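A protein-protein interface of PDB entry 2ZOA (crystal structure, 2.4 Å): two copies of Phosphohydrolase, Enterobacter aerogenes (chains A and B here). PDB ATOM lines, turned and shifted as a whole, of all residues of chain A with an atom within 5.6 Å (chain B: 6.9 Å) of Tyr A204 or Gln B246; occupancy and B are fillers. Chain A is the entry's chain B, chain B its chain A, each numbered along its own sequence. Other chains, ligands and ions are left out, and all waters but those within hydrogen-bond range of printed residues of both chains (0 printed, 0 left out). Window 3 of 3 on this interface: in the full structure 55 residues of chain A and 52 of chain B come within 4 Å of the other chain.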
ATOM      1  N   LEU A 160       2.442  -8.751  -5.484  1.00  0.00           N
ATOM      2  CA  LEU A 160       2.228 -10.133  -5.027  1.00  0.00           C
ATOM      3  C   LEU A 160       0.976 -10.683  -5.665  1.00  0.00           C
ATOM      4  O   LEU A 160       0.144  -9.909  -6.133  1.00  0.00           O
ATOM      5  CB  LEU A 160       2.182 -10.265  -3.478  1.00  0.00           C
ATOM      6  CG  LEU A 160       1.039  -9.674  -2.629  1.00  0.00           C
ATOM      7  CD1 LEU A 160       1.355  -9.795  -1.167  1.00  0.00           C
ATOM      8  CD2 LEU A 160       0.761  -8.219  -2.975  1.00  0.00           C
ATOM      9  N   PRO A 161       0.875 -12.028  -5.737  1.00  0.00           N
ATOM     10  CA  PRO A 161      -0.348 -12.686  -6.231  1.00  0.00           C
ATOM     11  C   PRO A 161      -1.519 -12.462  -5.271  1.00  0.00           C
ATOM     12  O   PRO A 161      -1.360 -12.606  -4.063  1.00  0.00           O
ATOM     13  CB  PRO A 161       0.040 -14.173  -6.265  1.00  0.00           C
ATOM     14  CG  PRO A 161       1.179 -14.296  -5.277  1.00  0.00           C
ATOM     15  CD  PRO A 161       1.932 -13.008  -5.398  1.00  0.00           C
ATOM     16  N   LEU A 179       8.428  -6.487  -1.911  1.00  0.00           N
ATOM     17  CA  LEU A 179       8.187  -7.140  -0.620  1.00  0.00           C
ATOM     18  C   LEU A 179       9.424  -7.111   0.306  1.00  0.00           C
ATOM     19  O   LEU A 179       9.311  -6.839   1.513  1.00  0.00           O
ATOM     20  CB  LEU A 179       7.728  -8.582  -0.878  1.00  0.00           C
ATOM     21  CG  LEU A 179       6.217  -8.926  -0.898  1.00  0.00           C
ATOM     22  CD1 LEU A 179       5.313  -7.774  -1.292  1.00  0.00           C
ATOM     23  CD2 LEU A 179       5.885 -10.247  -1.661  1.00  0.00           C
ATOM     24  N   VAL A 182       9.729  -3.735   1.768  1.00  0.00           N
ATOM     25  CA  VAL A 182       8.839  -3.440   2.900  1.00  0.00           C
ATOM     26  C   VAL A 182       9.372  -4.081   4.179  1.00  0.00           C
ATOM     27  O   VAL A 182       9.254  -3.492   5.255  1.00  0.00           O
ATOM     28  CB  VAL A 182       7.283  -3.704   2.687  1.00  0.00           C
ATOM     29  CG1 VAL A 182       6.835  -3.553   1.212  1.00  0.00           C
ATOM     30  CG2 VAL A 182       6.815  -5.013   3.290  1.00  0.00           C
ATOM     31  N   GLU A 183       9.970  -5.263   4.060  1.00  0.00           N
ATOM     32  CA  GLU A 183      10.715  -5.873   5.171  1.00  0.00           C
ATOM     33  C   GLU A 183      11.904  -5.047   5.675  1.00  0.00           C
ATOM     34  O   GLU A 183      12.079  -4.952   6.861  1.00  0.00           O
ATOM     35  CB  GLU A 183      11.157  -7.309   4.840  1.00  0.00           C
ATOM     36  CG  GLU A 183      10.000  -8.226   4.417  1.00  0.00           C
ATOM     37  CD  GLU A 183      10.381  -9.706   4.360  1.00  0.00           C
ATOM     38  OE1 GLU A 183       9.523 -10.529   3.972  1.00  0.00           O
ATOM     39  OE2 GLU A 183      11.532 -10.059   4.704  1.00  0.00           O
ATOM     40  N   THR A 202      -4.771  -5.901   0.567  1.00  0.00           N
ATOM     41  CA  THR A 202      -4.101  -6.826   1.456  1.00  0.00           C
ATOM     42  C   THR A 202      -3.037  -6.072   2.267  1.00  0.00           C
ATOM     43  O   THR A 202      -2.871  -4.866   2.111  1.00  0.00           O
ATOM     44  CB  THR A 202      -3.543  -8.054   0.666  1.00  0.00           C
ATOM     45  OG1 THR A 202      -3.252  -9.124   1.574  1.00  0.00           O
ATOM     46  CG2 THR A 202      -2.313  -7.689  -0.204  1.00  0.00           C
ATOM     47  N   GLN A 203      -2.361  -6.779   3.143  1.00  0.00           N
ATOM     48  CA  GLN A 203      -1.416  -6.205   4.075  1.00  0.00           C
ATOM     49  C   GLN A 203      -0.196  -7.108   4.111  1.00  0.00           C
ATOM     50  O   GLN A 203      -0.316  -8.285   4.226  1.00  0.00           O
ATOM     51  CB  GLN A 203      -2.086  -6.088   5.448  1.00  0.00           C
ATOM     52  CG  GLN A 203      -1.188  -5.915   6.631  1.00  0.00           C
ATOM     53  CD  GLN A 203      -0.675  -7.237   7.283  1.00  0.00           C
ATOM     54  OE1 GLN A 203      -1.230  -8.315   7.109  1.00  0.00           O
ATOM     55  NE2 GLN A 203       0.400  -7.114   8.033  1.00  0.00           N
ATOM     56  N   TYR A 204       0.981  -6.545   3.956  1.00  0.00           N
ATOM     57  CA  TYR A 204       2.231  -7.280   4.152  1.00  0.00           C
ATOM     58  C   TYR A 204       3.074  -6.484   5.145  1.00  0.00           C
ATOM     59  O   TYR A 204       3.443  -5.346   4.859  1.00  0.00           O
ATOM     60  CB  TYR A 204       2.952  -7.432   2.819  1.00  0.00           C
ATOM     61  CG  TYR A 204       4.080  -8.413   2.864  1.00  0.00           C
ATOM     62  CD1 TYR A 204       3.850  -9.776   2.662  1.00  0.00           C
ATOM     63  CD2 TYR A 204       5.384  -7.988   3.142  1.00  0.00           C
ATOM     64  CE1 TYR A 204       4.905 -10.696   2.715  1.00  0.00           C
ATOM     65  CE2 TYR A 204       6.433  -8.879   3.195  1.00  0.00           C
ATOM     66  CZ  TYR A 204       6.197 -10.235   2.979  1.00  0.00           C
ATOM     67  OH  TYR A 204       7.263 -11.125   3.045  1.00  0.00           O
ATOM     68  N   ARG A 205       3.380  -7.085   6.299  1.00  0.00           N
ATOM     69  CA  ARG A 205       3.947  -6.365   7.462  1.00  0.00           C
ATOM     70  C   ARG A 205       3.180  -5.030   7.699  1.00  0.00           C
ATOM     71  O   ARG A 205       1.959  -5.036   7.873  1.00  0.00           O
ATOM     72  CB  ARG A 205       5.476  -6.166   7.344  1.00  0.00           C
ATOM     73  CG  ARG A 205       6.256  -7.354   6.737  1.00  0.00           C
ATOM     74  CD  ARG A 205       6.422  -8.510   7.689  1.00  0.00           C
ATOM     75  NE  ARG A 205       7.840  -8.691   7.987  1.00  0.00           N
ATOM     76  CZ  ARG A 205       8.555  -9.756   7.630  1.00  0.00           C
ATOM     77  NH1 ARG A 205       7.995 -10.773   6.979  1.00  0.00           N
ATOM     78  NH2 ARG A 205       9.827  -9.806   7.921  1.00  0.00           N
ATOM     79  N   GLN A 206       3.880  -3.902   7.661  1.00  0.00           N
ATOM     80  CA  GLN A 206       3.264  -2.590   7.886  1.00  0.00           C
ATOM     81  C   GLN A 206       2.740  -1.940   6.593  1.00  0.00           C
ATOM     82  O   GLN A 206       2.170  -0.844   6.638  1.00  0.00           O
ATOM     83  CB  GLN A 206       4.262  -1.651   8.594  1.00  0.00           C
ATOM     84  CG  GLN A 206       5.367  -1.009   7.685  1.00  0.00           C
ATOM     85  CD  GLN A 206       6.415  -1.993   7.154  1.00  0.00           C
ATOM     86  OE1 GLN A 206       7.063  -1.741   6.134  1.00  0.00           O
ATOM     87  NE2 GLN A 206       6.576  -3.111   7.832  1.00  0.00           N
ATOM     88  N   ALA A 207       2.936  -2.587   5.442  1.00  0.00           N
ATOM     89  CA  ALA A 207       2.366  -2.050   4.199  1.00  0.00           C
ATOM     90  C   ALA A 207       0.931  -2.543   3.869  1.00  0.00           C
ATOM     91  O   ALA A 207       0.655  -3.762   3.794  1.00  0.00           O
ATOM     92  CB  ALA A 207       3.286  -2.268   3.019  1.00  0.00           C
ATOM     93  N   LEU A 208       0.033  -1.571   3.697  1.00  0.00           N
ATOM     94  CA  LEU A 208      -1.229  -1.767   3.022  1.00  0.00           C
ATOM     95  C   LEU A 208      -0.984  -1.710   1.509  1.00  0.00           C
ATOM     96  O   LEU A 208      -0.339  -0.794   1.003  1.00  0.00           O
ATOM     97  CB  LEU A 208      -2.254  -0.754   3.543  1.00  0.00           C
ATOM     98  CG  LEU A 208      -3.574  -0.220   2.951  1.00  0.00           C
ATOM     99  CD1 LEU A 208      -4.018  -0.708   1.558  1.00  0.00           C
ATOM    100  CD2 LEU A 208      -4.693  -0.266   3.951  1.00  0.00           C
ATOM    101  N   ILE A 209      -1.422  -2.753   0.819  1.00  0.00           N
ATOM    102  CA  ILE A 209      -1.189  -2.900  -0.619  1.00  0.00           C
ATOM    103  C   ILE A 209      -2.553  -3.050  -1.277  1.00  0.00           C
ATOM    104  O   ILE A 209      -3.309  -3.974  -0.937  1.00  0.00           O
ATOM    105  CB  ILE A 209      -0.343  -4.146  -0.943  1.00  0.00           C
ATOM    106  CG1 ILE A 209       0.976  -4.107  -0.167  1.00  0.00           C
ATOM    107  CG2 ILE A 209      -0.160  -4.285  -2.474  1.00  0.00           C
ATOM    108  CD1 ILE A 209       1.818  -5.374  -0.234  1.00  0.00           C
ATOM    109  N   THR B 114      -6.886 -18.008   9.809  1.00  0.00           N
ATOM    110  CA  THR B 114      -6.935 -16.758  10.567  1.00  0.00           C
ATOM    111  C   THR B 114      -8.083 -16.870  11.567  1.00  0.00           C
ATOM    112  O   THR B 114      -9.175 -17.290  11.201  1.00  0.00           O
ATOM    113  CB  THR B 114      -7.156 -15.555   9.614  1.00  0.00           C
ATOM    114  OG1 THR B 114      -6.039 -15.448   8.724  1.00  0.00           O
ATOM    115  CG2 THR B 114      -7.304 -14.238  10.371  1.00  0.00           C
ATOM    116  N   ARG B 190      -6.179  -7.389  10.934  1.00  0.00           N
ATOM    117  CA  ARG B 190      -7.340  -6.873  10.216  1.00  0.00           C
ATOM    118  C   ARG B 190      -8.367  -6.442  11.231  1.00  0.00           C
ATOM    119  O   ARG B 190      -8.625  -7.158  12.211  1.00  0.00           O
ATOM    120  CB  ARG B 190      -8.032  -7.911   9.321  1.00  0.00           C
ATOM    121  CG  ARG B 190      -7.404  -8.450   8.016  1.00  0.00           C
ATOM    122  CD  ARG B 190      -7.043  -7.448   6.881  1.00  0.00           C
ATOM    123  NE  ARG B 190      -5.637  -7.455   7.032  1.00  0.00           N
ATOM    124  CZ  ARG B 190      -4.724  -8.107   6.332  1.00  0.00           C
ATOM    125  NH1 ARG B 190      -4.970  -8.692   5.182  1.00  0.00           N
ATOM    126  NH2 ARG B 190      -3.498  -8.045   6.808  1.00  0.00           N
ATOM    127  N   GLN B 203      -4.105   1.924   7.579  1.00  0.00           N
ATOM    128  CA  GLN B 203      -3.262   0.945   8.239  1.00  0.00           C
ATOM    129  C   GLN B 203      -2.702   1.523   9.525  1.00  0.00           C
ATOM    130  O   GLN B 203      -2.295   2.641   9.549  1.00  0.00           O
ATOM    131  CB  GLN B 203      -2.169   0.431   7.291  1.00  0.00           C
ATOM    132  CG  GLN B 203      -1.285  -0.696   7.833  1.00  0.00           C
ATOM    133  CD  GLN B 203      -1.444  -2.056   7.125  1.00  0.00           C
ATOM    134  OE1 GLN B 203      -0.639  -2.946   7.294  1.00  0.00           O
ATOM    135  NE2 GLN B 203      -2.487  -2.205   6.358  1.00  0.00           N
ATOM    136  N   GLN B 206       0.687  -3.159  11.986  1.00  0.00           N
ATOM    137  CA  GLN B 206       0.381  -4.274  11.062  1.00  0.00           C
ATOM    138  C   GLN B 206      -1.073  -4.422  10.705  1.00  0.00           C
ATOM    139  O   GLN B 206      -1.424  -5.280   9.892  1.00  0.00           O
ATOM    140  CB  GLN B 206       0.834  -5.654  11.561  1.00  0.00           C
ATOM    141  CG  GLN B 206       1.318  -5.866  12.961  1.00  0.00           C
ATOM    142  CD  GLN B 206       0.564  -5.225  14.098  1.00  0.00           C
ATOM    143  OE1 GLN B 206      -0.483  -5.681  14.529  1.00  0.00           O
ATOM    144  NE2 GLN B 206       1.181  -4.225  14.675  1.00  0.00           N
ATOM    145  N   ARG B 241     -10.751 -13.533   1.289  1.00  0.00           N
ATOM    146  CA  ARG B 241     -10.201 -14.836   0.936  1.00  0.00           C
ATOM    147  C   ARG B 241      -8.823 -15.050   1.531  1.00  0.00           C
ATOM    148  O   ARG B 241      -7.996 -14.137   1.543  1.00  0.00           O
ATOM    149  CB  ARG B 241     -10.102 -14.978  -0.583  1.00  0.00           C
ATOM    150  CG  ARG B 241      -9.900 -16.411  -1.022  1.00  0.00           C
ATOM    151  CD  ARG B 241      -9.663 -16.574  -2.495  1.00  0.00           C
ATOM    152  NE  ARG B 241     -10.851 -16.263  -3.282  1.00  0.00           N
ATOM    153  CZ  ARG B 241     -11.803 -17.142  -3.635  1.00  0.00           C
ATOM    154  NH1 ARG B 241     -11.705 -18.429  -3.233  1.00  0.00           N
ATOM    155  NH2 ARG B 241     -12.846 -16.725  -4.401  1.00  0.00           N
ATOM    156  N   GLN B 242      -8.565 -16.256   2.021  1.00  0.00           N
ATOM    157  CA  GLN B 242      -7.223 -16.610   2.463  1.00  0.00           C
ATOM    158  C   GLN B 242      -6.453 -17.152   1.264  1.00  0.00           C
ATOM    159  O   GLN B 242      -6.820 -18.180   0.714  1.00  0.00           O
ATOM    160  CB  GLN B 242      -7.278 -17.642   3.574  1.00  0.00           C
ATOM    161  CG  GLN B 242      -5.937 -17.927   4.212  1.00  0.00           C
ATOM    162  CD  GLN B 242      -5.476 -16.822   5.178  1.00  0.00           C
ATOM    163  OE1 GLN B 242      -4.317 -16.380   5.131  1.00  0.00           O
ATOM    164  NE2 GLN B 242      -6.376 -16.401   6.078  1.00  0.00           N
ATOM    165  N   VAL B 243      -5.405 -16.437   0.852  1.00  0.00           N
ATOM    166  CA  VAL B 243      -4.590 -16.795  -0.312  1.00  0.00           C
ATOM    167  C   VAL B 243      -3.174 -17.084   0.171  1.00  0.00           C
ATOM    168  O   VAL B 243      -2.352 -16.175   0.279  1.00  0.00           O
ATOM    169  CB  VAL B 243      -4.609 -15.660  -1.407  1.00  0.00           C
ATOM    170  CG1 VAL B 243      -3.774 -16.043  -2.645  1.00  0.00           C
ATOM    171  CG2 VAL B 243      -6.012 -15.358  -1.806  1.00  0.00           C
ATOM    172  N   GLY B 244      -2.893 -18.347   0.481  1.00  0.00           N
ATOM    173  CA  GLY B 244      -1.653 -18.700   1.176  1.00  0.00           C
ATOM    174  C   GLY B 244      -1.605 -17.962   2.501  1.00  0.00           C
ATOM    175  O   GLY B 244      -2.534 -18.061   3.306  1.00  0.00           O
ATOM    176  N   GLU B 245      -0.543 -17.183   2.702  1.00  0.00           N
ATOM    177  CA  GLU B 245      -0.320 -16.428   3.943  1.00  0.00           C
ATOM    178  C   GLU B 245      -1.073 -15.091   3.987  1.00  0.00           C
ATOM    179  O   GLU B 245      -1.134 -14.442   5.039  1.00  0.00           O
ATOM    180  CB  GLU B 245       1.174 -16.163   4.105  1.00  0.00           C
ATOM    181  CG  GLU B 245       1.752 -16.528   5.503  1.00  0.00           C
ATOM    182  CD  GLU B 245       1.718 -18.048   5.860  1.00  0.00           C
ATOM    183  OE1 GLU B 245       2.354 -18.427   6.884  1.00  0.00           O
ATOM    184  OE2 GLU B 245       1.069 -18.857   5.137  1.00  0.00           O
ATOM    185  N   GLN B 246      -1.622 -14.685   2.840  1.00  0.00           N
ATOM    186  CA  GLN B 246      -2.272 -13.392   2.669  1.00  0.00           C
ATOM    187  C   GLN B 246      -3.780 -13.473   2.861  1.00  0.00           C
ATOM    188  O   GLN B 246      -4.448 -14.325   2.269  1.00  0.00           O
ATOM    189  CB  GLN B 246      -1.975 -12.827   1.265  1.00  0.00           C
ATOM    190  CG  GLN B 246      -0.493 -12.508   1.040  1.00  0.00           C
ATOM    191  CD  GLN B 246       0.020 -11.536   2.091  1.00  0.00           C
ATOM    192  OE1 GLN B 246      -0.615 -10.501   2.352  1.00  0.00           O
ATOM    193  NE2 GLN B 246       1.138 -11.864   2.719  1.00  0.00           N
ATOM    194  N   TRP B 247      -4.297 -12.592   3.715  1.00  0.00           N
ATOM    195  CA  TRP B 247      -5.710 -12.286   3.746  1.00  0.00           C
ATOM    196  C   TRP B 247      -5.952 -11.195   2.698  1.00  0.00           C
ATOM    197  O   TRP B 247      -5.390 -10.090   2.781  1.00  0.00           O
ATOM    198  CB  TRP B 247      -6.105 -11.809   5.134  1.00  0.00           C
ATOM    199  CG  TRP B 247      -7.549 -11.427   5.284  1.00  0.00           C
ATOM    200  CD1 TRP B 247      -8.214 -10.435   4.615  1.00  0.00           C
ATOM    201  CD2 TRP B 247      -8.505 -12.029   6.166  1.00  0.00           C
ATOM    202  NE1 TRP B 247      -9.522 -10.383   5.023  1.00  0.00           N
ATOM    203  CE2 TRP B 247      -9.732 -11.341   5.981  1.00  0.00           C
ATOM    204  CE3 TRP B 247      -8.452 -13.091   7.082  1.00  0.00           C
ATOM    205  CZ2 TRP B 247     -10.890 -11.669   6.691  1.00  0.00           C
ATOM    206  CZ3 TRP B 247      -9.598 -13.420   7.778  1.00  0.00           C
ATOM    207  CH2 TRP B 247     -10.811 -12.704   7.576  1.00  0.00           C
ATOM    208  N   VAL B 248      -6.772 -11.524   1.704  1.00  0.00           N
ATOM    209  CA  VAL B 248      -7.073 -10.621   0.606  1.00  0.00           C
ATOM    210  C   VAL B 248      -8.567 -10.274   0.650  1.00  0.00           C
ATOM    211  O   VAL B 248      -9.415 -11.162   0.842  1.00  0.00           O
ATOM    212  CB  VAL B 248      -6.711 -11.291  -0.762  1.00  0.00           C
ATOM    213  CG1 VAL B 248      -7.046 -10.388  -1.921  1.00  0.00           C
ATOM    214  CG2 VAL B 248      -5.221 -11.728  -0.786  1.00  0.00           C
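OE1 of Gln A203 sits close to NH2 of Arg B190 (2.3 Å).
The backbone carbonyl oxygen (O) of Trp B247 is in hydrogen-bond range of the side-chain hydroxyl (OG1) of Thr A202 (2.6 Å).
The backbone carbonyl oxygen (O) of Gln B206 sits at hydrogen-bond distance from the side-chain amide nitrogen (NE2) of Gln A203 (3.2 Å).
OE1 of Gln B203 lies close to O of Arg A205, at 3.4 Å.
The side-chain amide oxygen (OE1) of Gln B246 sits close to the backbone carbonyl oxygen (O) of Gln A203 (2.9 Å).
The side-chain amide oxygen (OE1) of Gln B246 sits at hydrogen-bond distance from the side-chain hydroxyl (OG1) of Thr A202.
The guanidinium group (NH1) of Arg B190 sits at hydrogen-bond distance from the backbone carbonyl oxygen (O) of Trp B247 (2.8 Å).
The side-chain carboxylate (OE1) of Glu A183 is in hydrogen-bond range of the side-chain hydroxyl (OH) of Tyr A204 (2.5 Å).
The guanidinium group of Arg A205 is in salt-bridge range of the side-chain carboxylate of Glu A183, at 3.4 Å.
O of Arg A205 sits at hydrogen-bond distance from NE2 of Gln A203.
OE1 of Gln A206 sits close to O of Val A182, 2.9 Å away.
The backbone NH of Thr A202 is in hydrogen-bond range of the backbone carbonyl oxygen of Ile A209, 2.8 Å away.
Printed residues of chain B that touch a printed residue of chain A: Arg B190, Gln B203, Gln B206, Gln B246 and Trp B247.
Hydrophobic or aromatic side chains of chain A within 4 Å of the printed part of chain B: Leu A160, Tyr A204 and Leu A208.
Among the printed residues, no Asp or Glu carboxylate lies within 4 Å of a Lys or Arg side-chain nitrogen of the other chain.
CD1 of Leu A160 touches CD of Gln B246, at 3.9 Å.
CG of Gln A203 touches OE1 of Gln B203, at 3.1 Å.
NE2 of Gln B246 touches CD1 of Tyr A204, at 3.4 Å.
Gln B206 touches Arg A205 (CA to O, 3.6 Å).
Gln B203 touches Gln A206.
Ala A207 touches Gln B203 (C to OE1, 3.8 Å).
Leu A208 touches Gln B203 (CB to NE2, 3.2 Å).
Of chain A, only Leu A160 (3.9 Å), Thr A202 (3.1 Å), Gln A203 (2.9 Å) and Tyr A204 (3.4 Å) come within 4 Å of Gln B246.
Printed residues of chain A within 4 Å of Trp B247: Thr A202 (2.6 Å).
Of the printed residues of chain B, Leu A160 touches Gln B246.
Printed residues of chain B within 4 Å of Gln A206: Gln B203 (3.6 Å).
Pro A161 touches none of the printed residues of chain B.
Ile A209 touches none of the printed residues of chain B.
Gln B203 touches its own counterpart, Gln A203.
Gln A203 touches Gln B206, and with the chains exchanged Gln A206 touches Gln B203.
Positions printed for both chains: 203 and 206.
Of the 13 pairs that touch across the chains among the printed residues, 3 have their exchanged pair printed and touching as well.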
